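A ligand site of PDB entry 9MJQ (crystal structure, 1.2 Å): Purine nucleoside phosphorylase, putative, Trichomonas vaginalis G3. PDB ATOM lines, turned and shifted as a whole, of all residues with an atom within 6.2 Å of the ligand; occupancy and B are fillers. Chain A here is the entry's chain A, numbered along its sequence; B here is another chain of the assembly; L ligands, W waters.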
ATOM      1  N   GLY A  29       8.035  -7.960  -1.965  1.00  0.00           N
ATOM      2  CA  GLY A  29       9.040  -8.890  -2.460  1.00  0.00           C
ATOM      3  C   GLY A  29       9.804  -8.357  -3.649  1.00  0.00           C
ATOM      4  O   GLY A  29      11.016  -8.545  -3.750  1.00  0.00           O
ATOM      5  N   HIS A  71      12.135  -7.060  -0.477  1.00  0.00           N
ATOM      6  CA  HIS A  71      12.628  -8.066   0.457  1.00  0.00           C
ATOM      7  C   HIS A  71      12.988  -9.398  -0.180  1.00  0.00           C
ATOM      8  O   HIS A  71      13.500 -10.264   0.534  1.00  0.00           O
ATOM      9  CB  HIS A  71      11.699  -8.266   1.690  1.00  0.00           C
ATOM     10  CG  HIS A  71      10.296  -8.727   1.387  1.00  0.00           C
ATOM     11  ND1 HIS A  71      10.003  -9.879   0.693  1.00  0.00           N
ATOM     12  CD2 HIS A  71       9.106  -8.205   1.762  1.00  0.00           C
ATOM     13  CE1 HIS A  71       8.688 -10.034   0.643  1.00  0.00           C
ATOM     14  NE2 HIS A  71       8.119  -9.035   1.282  1.00  0.00           N
ATOM     15  N   GLY A  72      12.750  -9.590  -1.488  1.00  0.00           N
ATOM     16  CA  GLY A  72      13.019 -10.873  -2.124  1.00  0.00           C
ATOM     17  C   GLY A  72      11.976 -11.904  -1.753  1.00  0.00           C
ATOM     18  O   GLY A  72      11.030 -11.633  -1.035  1.00  0.00           O
ATOM     19  N   MET A  73      12.168 -13.125  -2.219  1.00  0.00           N
ATOM     20  CA  MET A  73      11.209 -14.192  -1.978  1.00  0.00           C
ATOM     21  C   MET A  73      11.716 -15.158  -0.926  1.00  0.00           C
ATOM     22  O   MET A  73      12.829 -15.681  -1.029  1.00  0.00           O
ATOM     23  CB  MET A  73      10.880 -14.940  -3.269  1.00  0.00           C
ATOM     24  CG  MET A  73      10.302 -14.029  -4.355  1.00  0.00           C
ATOM     25  SD  MET A  73       9.591 -14.871  -5.752  1.00  0.00           S
ATOM     26  CE  MET A  73      11.074 -15.488  -6.504  1.00  0.00           C
ATOM     27  N   GLY A  74      10.897 -15.387   0.084  1.00  0.00           N
ATOM     28  CA  GLY A  74      11.120 -16.423   1.068  1.00  0.00           C
ATOM     29  C   GLY A  74      11.578 -15.893   2.422  1.00  0.00           C
ATOM     30  O   GLY A  74      12.153 -14.800   2.554  1.00  0.00           O
ATOM     31  N   ARG A  96       4.684  -5.434   5.677  1.00  0.00           N
ATOM     32  CA  ARG A  96       4.862  -6.183   4.454  1.00  0.00           C
ATOM     33  C   ARG A  96       3.625  -5.995   3.583  1.00  0.00           C
ATOM     34  O   ARG A  96       2.498  -6.135   4.054  1.00  0.00           O
ATOM     35  CB  ARG A  96       5.104  -7.653   4.757  1.00  0.00           C
ATOM     36  CG  ARG A  96       5.815  -8.318   3.647  1.00  0.00           C
ATOM     37  CD  ARG A  96       6.035  -9.774   3.852  1.00  0.00           C
ATOM     38  NE  ARG A  96       4.925 -10.550   3.341  1.00  0.00           N
ATOM     39  CZ  ARG A  96       4.617 -10.704   2.069  1.00  0.00           C
ATOM     40  NH1 ARG A  96       5.331 -10.130   1.111  1.00  0.00           N
ATOM     41  NH2 ARG A  96       3.579 -11.454   1.734  1.00  0.00           N
ATOM     42  N   GLY A  98       2.076  -7.211  -0.164  1.00  0.00           N
ATOM     43  CA  GLY A  98       2.394  -8.213  -1.139  1.00  0.00           C
ATOM     44  C   GLY A  98       1.175  -8.828  -1.778  1.00  0.00           C
ATOM     45  O   GLY A  98       0.069  -8.314  -1.660  1.00  0.00           O
ATOM     46  N   THR A  99       1.412  -9.928  -2.479  1.00  0.00           N
ATOM     47  CA  THR A  99       0.382 -10.732  -3.105  1.00  0.00           C
ATOM     48  C   THR A  99       0.369 -12.106  -2.450  1.00  0.00           C
ATOM     49  O   THR A  99       1.309 -12.510  -1.763  1.00  0.00           O
ATOM     50  CB  THR A  99       0.650 -10.868  -4.602  1.00  0.00           C
ATOM     51  OG1 THR A  99       1.848 -11.642  -4.779  1.00  0.00           O
ATOM     52  CG2 THR A  99       0.805  -9.488  -5.250  1.00  0.00           C
ATOM     53  N   CYS A 100      -0.726 -12.825  -2.679  1.00  0.00           N
ATOM     54  CA  CYS A 100      -0.865 -14.146  -2.084  1.00  0.00           C
ATOM     55  C   CYS A 100      -1.803 -14.989  -2.924  1.00  0.00           C
ATOM     56  O   CYS A 100      -2.555 -14.483  -3.747  1.00  0.00           O
ATOM     57  CB  CYS A 100      -1.397 -14.044  -0.651  1.00  0.00           C
ATOM     58  SG  CYS A 100      -3.068 -13.355  -0.507  1.00  0.00           S
ATOM     59  N   GLY A 101      -1.774 -16.295  -2.674  1.00  0.00           N
ATOM     60  CA  GLY A 101      -2.819 -17.187  -3.118  1.00  0.00           C
ATOM     61  C   GLY A 101      -3.817 -17.404  -1.990  1.00  0.00           C
ATOM     62  O   GLY A 101      -3.592 -16.976  -0.866  1.00  0.00           O
ATOM     63  N   THR A 102      -4.923 -18.055  -2.299  1.00  0.00           N
ATOM     64  CA  THR A 102      -5.847 -18.470  -1.253  1.00  0.00           C
ATOM     65  C   THR A 102      -6.411 -19.843  -1.585  1.00  0.00           C
ATOM     66  O   THR A 102      -6.544 -20.212  -2.750  1.00  0.00           O
ATOM     67  CB  THR A 102      -6.994 -17.464  -1.037  1.00  0.00           C
ATOM     68  OG1 THR A 102      -7.694 -17.791   0.162  1.00  0.00           O
ATOM     69  CG2 THR A 102      -7.981 -17.497  -2.191  1.00  0.00           C
ATOM     70  N   THR A 165       5.028 -20.370   3.279  1.00  0.00           N
ATOM     71  CA  THR A 165       5.699 -21.600   2.898  1.00  0.00           C
ATOM     72  C   THR A 165       7.094 -21.320   2.311  1.00  0.00           C
ATOM     73  O   THR A 165       7.335 -20.300   1.670  1.00  0.00           O
ATOM     74  CB  THR A 165       4.857 -22.411   1.905  1.00  0.00           C
ATOM     75  OG1 THR A 165       5.515 -23.653   1.625  1.00  0.00           O
ATOM     76  CG2 THR A 165       4.622 -21.666   0.609  1.00  0.00           C
ATOM     77  N   ILE A 167       8.101 -23.432   0.054  1.00  0.00           N
ATOM     78  CA  ILE A 167       8.002 -24.153  -1.212  1.00  0.00           C
ATOM     79  C   ILE A 167       6.838 -23.590  -2.014  1.00  0.00           C
ATOM     80  O   ILE A 167       5.683 -23.962  -1.813  1.00  0.00           O
ATOM     81  CB  ILE A 167       7.903 -25.668  -1.028  1.00  0.00           C
ATOM     82  CG1 ILE A 167       9.217 -26.199  -0.435  1.00  0.00           C
ATOM     83  CG2 ILE A 167       7.557 -26.353  -2.355  1.00  0.00           C
ATOM     84  CD1 ILE A 167      10.426 -26.105  -1.375  1.00  0.00           C
ATOM     85  N   PHE A 168       7.152 -22.701  -2.952  1.00  0.00           N
ATOM     86  CA  PHE A 168       6.123 -22.213  -3.866  1.00  0.00           C
ATOM     87  C   PHE A 168       5.475 -23.350  -4.623  1.00  0.00           C
ATOM     88  O   PHE A 168       4.245 -23.437  -4.726  1.00  0.00           O
ATOM     89  CB  PHE A 168       6.740 -21.192  -4.810  1.00  0.00           C
ATOM     90  CG  PHE A 168       5.749 -20.560  -5.760  1.00  0.00           C
ATOM     91  CD1 PHE A 168       5.067 -19.420  -5.390  1.00  0.00           C
ATOM     92  CD2 PHE A 168       5.499 -21.117  -7.000  1.00  0.00           C
ATOM     93  CE1 PHE A 168       4.148 -18.829  -6.247  1.00  0.00           C
ATOM     94  CE2 PHE A 168       4.591 -20.531  -7.865  1.00  0.00           C
ATOM     95  CZ  PHE A 168       3.898 -19.386  -7.487  1.00  0.00           C
ATOM     96  N   VAL A 187      -1.875 -17.470   1.306  1.00  0.00           N
ATOM     97  CA  VAL A 187      -0.675 -18.280   1.165  1.00  0.00           C
ATOM     98  C   VAL A 187       0.399 -17.398   0.554  1.00  0.00           C
ATOM     99  O   VAL A 187       0.227 -16.892  -0.565  1.00  0.00           O
ATOM    100  CB  VAL A 187      -0.928 -19.529   0.299  1.00  0.00           C
ATOM    101  CG1 VAL A 187       0.344 -20.366   0.194  1.00  0.00           C
ATOM    102  CG2 VAL A 187      -2.073 -20.349   0.866  1.00  0.00           C
ATOM    103  N   GLU A 188       1.494 -17.207   1.273  1.00  0.00           N
ATOM    104  CA  GLU A 188       2.621 -16.392   0.807  1.00  0.00           C
ATOM    105  C   GLU A 188       3.889 -17.067   1.317  1.00  0.00           C
ATOM    106  O   GLU A 188       3.881 -18.268   1.604  1.00  0.00           O
ATOM    107  CB  GLU A 188       2.390 -14.904   1.100  1.00  0.00           C
ATOM    108  CG  GLU A 188       1.905 -14.557   2.472  1.00  0.00           C
ATOM    109  CD  GLU A 188       2.974 -14.610   3.499  1.00  0.00           C
ATOM    110  OE1 GLU A 188       3.756 -13.670   3.635  1.00  0.00           O
ATOM    111  OE2 GLU A 188       3.074 -15.651   4.141  1.00  0.00           O
ATOM    112  N   MET A 189       5.000 -16.320   1.402  1.00  0.00           N
ATOM    113  CA  MET A 189       6.284 -16.953   1.710  1.00  0.00           C
ATOM    114  C   MET A 189       7.147 -16.175   2.702  1.00  0.00           C
ATOM    115  O   MET A 189       8.336 -16.506   2.841  1.00  0.00           O
ATOM    116  CB  MET A 189       7.100 -17.236   0.422  1.00  0.00           C
ATOM    117  CG  MET A 189       6.344 -18.124  -0.550  1.00  0.00           C
ATOM    118  SD  MET A 189       7.269 -18.472  -2.054  1.00  0.00           S
ATOM    119  CE  MET A 189       8.706 -19.318  -1.394  1.00  0.00           C
ATOM    120  N   GLU A 190       6.610 -15.195   3.431  1.00  0.00           N
ATOM    121  CA  GLU A 190       7.481 -14.295   4.163  1.00  0.00           C
ATOM    122  C   GLU A 190       7.037 -13.863   5.550  1.00  0.00           C
ATOM    123  O   GLU A 190       7.893 -13.665   6.422  1.00  0.00           O
ATOM    124  CB  GLU A 190       7.720 -13.031   3.323  1.00  0.00           C
ATOM    125  CG  GLU A 190       8.526 -13.227   2.056  1.00  0.00           C
ATOM    126  CD  GLU A 190       7.710 -13.670   0.851  1.00  0.00           C
ATOM    127  OE1 GLU A 190       6.451 -13.556   0.874  1.00  0.00           O
ATOM    128  OE2 GLU A 190       8.346 -14.115  -0.143  1.00  0.00           O
ATOM    129  N   SER A 212      -3.986 -12.919  -5.656  1.00  0.00           N
ATOM    130  CA  SER A 212      -3.769 -13.005  -7.099  1.00  0.00           C
ATOM    131  C   SER A 212      -4.384 -14.246  -7.715  1.00  0.00           C
ATOM    132  O   SER A 212      -4.799 -14.212  -8.881  1.00  0.00           O
ATOM    133  CB  SER A 212      -2.269 -13.086  -7.397  1.00  0.00           C
ATOM    134  OG  SER A 212      -1.598 -11.894  -7.063  1.00  0.00           O
ATOM    135  N   ASP A 213      -4.467 -15.348  -6.967  1.00  0.00           N
ATOM    136  CA  ASP A 213      -4.868 -16.621  -7.518  1.00  0.00           C
ATOM    137  C   ASP A 213      -5.623 -17.391  -6.460  1.00  0.00           C
ATOM    138  O   ASP A 213      -5.239 -17.386  -5.284  1.00  0.00           O
ATOM    139  CB  ASP A 213      -3.630 -17.444  -7.898  1.00  0.00           C
ATOM    140  CG  ASP A 213      -2.893 -16.869  -9.085  1.00  0.00           C
ATOM    141  OD1 ASP A 213      -3.326 -17.120 -10.228  1.00  0.00           O
ATOM    142  OD2 ASP A 213      -1.888 -16.159  -8.881  1.00  0.00           O
ATOM    143  N   ILE A 215      -6.100 -21.017  -5.408  1.00  0.00           N
ATOM    144  CA  ILE A 215      -5.385 -22.260  -5.636  1.00  0.00           C
ATOM    145  C   ILE A 215      -6.338 -23.421  -5.912  1.00  0.00           C
ATOM    146  O   ILE A 215      -5.964 -24.387  -6.589  1.00  0.00           O
ATOM    147  CB  ILE A 215      -4.465 -22.521  -4.432  1.00  0.00           C
ATOM    148  CG1 ILE A 215      -3.360 -21.456  -4.383  1.00  0.00           C
ATOM    149  CG2 ILE A 215      -3.861 -23.913  -4.482  1.00  0.00           C
ATOM    150  CD1 ILE A 215      -2.695 -21.316  -3.034  1.00  0.00           C
ATOM    151  N   PRO B  12       5.575 -17.410 -13.303  1.00  0.00           N
ATOM    152  CA  PRO B  12       5.305 -16.153 -12.603  1.00  0.00           C
ATOM    153  C   PRO B  12       6.536 -15.325 -12.347  1.00  0.00           C
ATOM    154  O   PRO B  12       6.418 -14.148 -11.995  1.00  0.00           O
ATOM    155  CB  PRO B  12       4.669 -16.610 -11.280  1.00  0.00           C
ATOM    156  CG  PRO B  12       4.195 -17.989 -11.529  1.00  0.00           C
ATOM    157  CD  PRO B  12       5.172 -18.585 -12.520  1.00  0.00           C
ATOM    158  N   HIS B  13       7.720 -15.894 -12.528  1.00  0.00           N
ATOM    159  CA  HIS B  13       8.960 -15.270 -12.091  1.00  0.00           C
ATOM    160  C   HIS B  13       9.966 -15.107 -13.225  1.00  0.00           C
ATOM    161  O   HIS B  13      11.084 -14.646 -12.984  1.00  0.00           O
ATOM    162  CB  HIS B  13       9.598 -16.096 -10.964  1.00  0.00           C
ATOM    163  CG  HIS B  13       8.632 -16.480  -9.893  1.00  0.00           C
ATOM    164  ND1 HIS B  13       8.052 -17.726  -9.829  1.00  0.00           N
ATOM    165  CD2 HIS B  13       8.119 -15.770  -8.861  1.00  0.00           C
ATOM    166  CE1 HIS B  13       7.228 -17.770  -8.788  1.00  0.00           C
ATOM    167  NE2 HIS B  13       7.239 -16.591  -8.193  1.00  0.00           N
ATOM    168  N   ARG B  52      11.336  -9.113 -11.479  1.00  0.00           N
ATOM    169  CA  ARG B  52      11.781  -8.912 -10.094  1.00  0.00           C
ATOM    170  C   ARG B  52      13.235  -8.493 -10.008  1.00  0.00           C
ATOM    171  O   ARG B  52      13.842  -8.579  -8.932  1.00  0.00           O
ATOM    172  CB  ARG B  52      11.487 -10.118  -9.201  1.00  0.00           C
ATOM    173  CG  ARG B  52      10.007 -10.365  -9.003  1.00  0.00           C
ATOM    174  CD  ARG B  52       9.717 -11.734  -8.377  1.00  0.00           C
ATOM    175  NE  ARG B  52       8.314 -11.902  -8.040  1.00  0.00           N
ATOM    176  CZ  ARG B  52       7.777 -11.628  -6.853  1.00  0.00           C
ATOM    177  NH1 ARG B  52       8.536 -11.189  -5.855  1.00  0.00           N
ATOM    178  NH2 ARG B  52       6.479 -11.830  -6.654  1.00  0.00           N
ATOM    179  N   ILE B  80      12.394 -21.792  -6.256  1.00  0.00           N
ATOM    180  CA  ILE B  80      11.520 -21.283  -7.315  1.00  0.00           C
ATOM    181  C   ILE B  80      12.254 -21.273  -8.651  1.00  0.00           C
ATOM    182  O   ILE B  80      11.773 -21.808  -9.661  1.00  0.00           O
ATOM    183  CB  ILE B  80      11.002 -19.874  -6.955  1.00  0.00           C
ATOM    184  CG1 ILE B  80       9.916 -19.965  -5.893  1.00  0.00           C
ATOM    185  CG2 ILE B  80      10.463 -19.145  -8.190  1.00  0.00           C
ATOM    186  CD1 ILE B  80       9.576 -18.645  -5.222  1.00  0.00           C
HETATM  187  N1  LIG L   1       2.925 -15.289  -3.470  1.00  0.00           N
HETATM  188  C1  LIG L   1       2.858 -16.634  -3.173  1.00  0.00           C
HETATM  189  N2  LIG L   1       3.720 -17.386  -2.455  1.00  0.00           N
HETATM  190  C2  LIG L   1       3.372 -18.629  -2.338  1.00  0.00           C
HETATM  191  N3  LIG L   1       2.254 -19.160  -2.882  1.00  0.00           N
HETATM  192  C3  LIG L   1       1.284 -18.465  -3.609  1.00  0.00           C
HETATM  193  O1  LIG L   1       0.292 -19.028  -4.045  1.00  0.00           O
HETATM  194  C4  LIG L   1       1.683 -17.094  -3.749  1.00  0.00           C
HETATM  195  N4  LIG L   1       1.051 -16.082  -4.398  1.00  0.00           N
HETATM  196  C5  LIG L   1       1.803 -15.057  -4.204  1.00  0.00           C
HETATM  197  C6  LIG L   1       5.825 -15.931  -5.117  1.00  0.00           C
HETATM  198  O2  LIG L   1       5.387 -15.681  -6.443  1.00  0.00           O
HETATM  199  C7  LIG L   1       5.915 -14.664  -4.312  1.00  0.00           C
HETATM  200  O3  LIG L   1       4.643 -13.975  -4.366  1.00  0.00           O
HETATM  201  C8  LIG L   1       3.926 -14.241  -3.189  1.00  0.00           C
HETATM  202  C9  LIG L   1       4.949 -14.538  -2.087  1.00  0.00           C
HETATM  203  O4  LIG L   1       5.055 -13.417  -1.223  1.00  0.00           O
HETATM  204  C10 LIG L   1       6.250 -14.844  -2.842  1.00  0.00           C
HETATM  205  O5  LIG L   1       7.261 -13.912  -2.466  1.00  0.00           O
HETATM  206  O   HOH W   1       4.476 -13.427  -8.146  1.00  0.00           O
HETATM  207  O   HOH W   2      -0.949 -19.152  -6.316  1.00  0.00           O
HETATM  208  O   HOH W   3       2.580 -22.004  -2.710  1.00  0.00           O
HETATM  209  O   HOH W   4       2.622 -15.794  -7.935  1.00  0.00           O
HETATM  210  O   HOH W   5       7.123 -11.369  -3.363  1.00  0.00           O
HETATM  211  O   HOH W   6       3.792 -11.186  -1.225  1.00  0.00           O
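An oxygen (O4) of the ligand is in hydrogen-bond range of the side-chain carboxylate of Glu 190.
A ring nitrogen (NE2) of His 13 of chain B is in hydrogen-bond range of an oxygen (O2) of the ligand (2.7 Å).
N of Gly 101 lies within hydrogen-bond range of N4 of the ligand (3.3 Å).
The backbone NH (N) of Glu 190 sits at hydrogen-bond distance from the side-chain carboxylate (OE1) of Glu 188 (3.2 Å).
OE1 of Glu 190 is in salt-bridge range of NH1 of Arg 96, at 3.6 Å.
The backbone NH of Gly 74 lies within hydrogen-bond range of the side-chain carboxylate of Glu 190 (2.9 Å).
The backbone carbonyl oxygen of Gly 101 is in hydrogen-bond range of the backbone NH of Val 187 (2.8 Å).
The backbone carbonyl oxygen (O) of Cys 100 lies within hydrogen-bond range of the backbone NH (N) of Ser 212 (2.9 Å).
The backbone carbonyl oxygen (O) of Glu 188 is in hydrogen-bond range of the backbone NH (N) of Thr 165, at 2.9 Å.
The guanidinium group (NH1) of Arg 96 is in hydrogen-bond range of a ring nitrogen (NE2) of His 71, 3.0 Å away.
The backbone carbonyl oxygen (O) of Thr 102 is in hydrogen-bond range of the backbone NH (N) of Ile 215, 2.8 Å away.
SD of Met 189 sits close to N2 of the ligand (3.7 Å).
CG of Met 73 touches O5 of the ligand (3.6 Å).
NH2 of Arg 96 touches O4 of the ligand (3.8 Å).
O of Thr 99 touches C8 of the ligand (3.4 Å).
Cys 100 touches the ligand (C to N4, 3.4 Å).
Phe 168 touches the ligand.
O of Val 187 touches C4 of the ligand (3.5 Å).
Glu 188 touches the ligand.
Ile 215 touches the ligand (CD1 to O1, 3.9 Å).
Arg 52 of chain B touches the ligand.
Hydrophobic or aromatic side chains that line the ligand: Met 73, Phe 168, Val 187, Met 189, Ile 215 and His 13 of chain B.
The nearest printed residue that does not touch the ligand is Thr 165 (4.4 Å).
Water W6 lies within hydrogen-bond range of an oxygen (O4) of the ligand (2.6 Å), the backbone carbonyl oxygen (O) of Thr 99 (2.9 Å) and the guanidinium group (NH2) of Arg 96 (3.0 Å).
Water W5 bridges an oxygen (O5) of the ligand and the guanidinium group (NH1) of Arg 52 of chain B.
Water W3 bridges a nitrogen (N3) of the ligand (2.9 Å) and the backbone carbonyl oxygen (O) of Phe 168 (3.0 Å).
Water W1 lies within hydrogen-bond range of NH2 of Arg 52 of chain B and O2 of the ligand.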
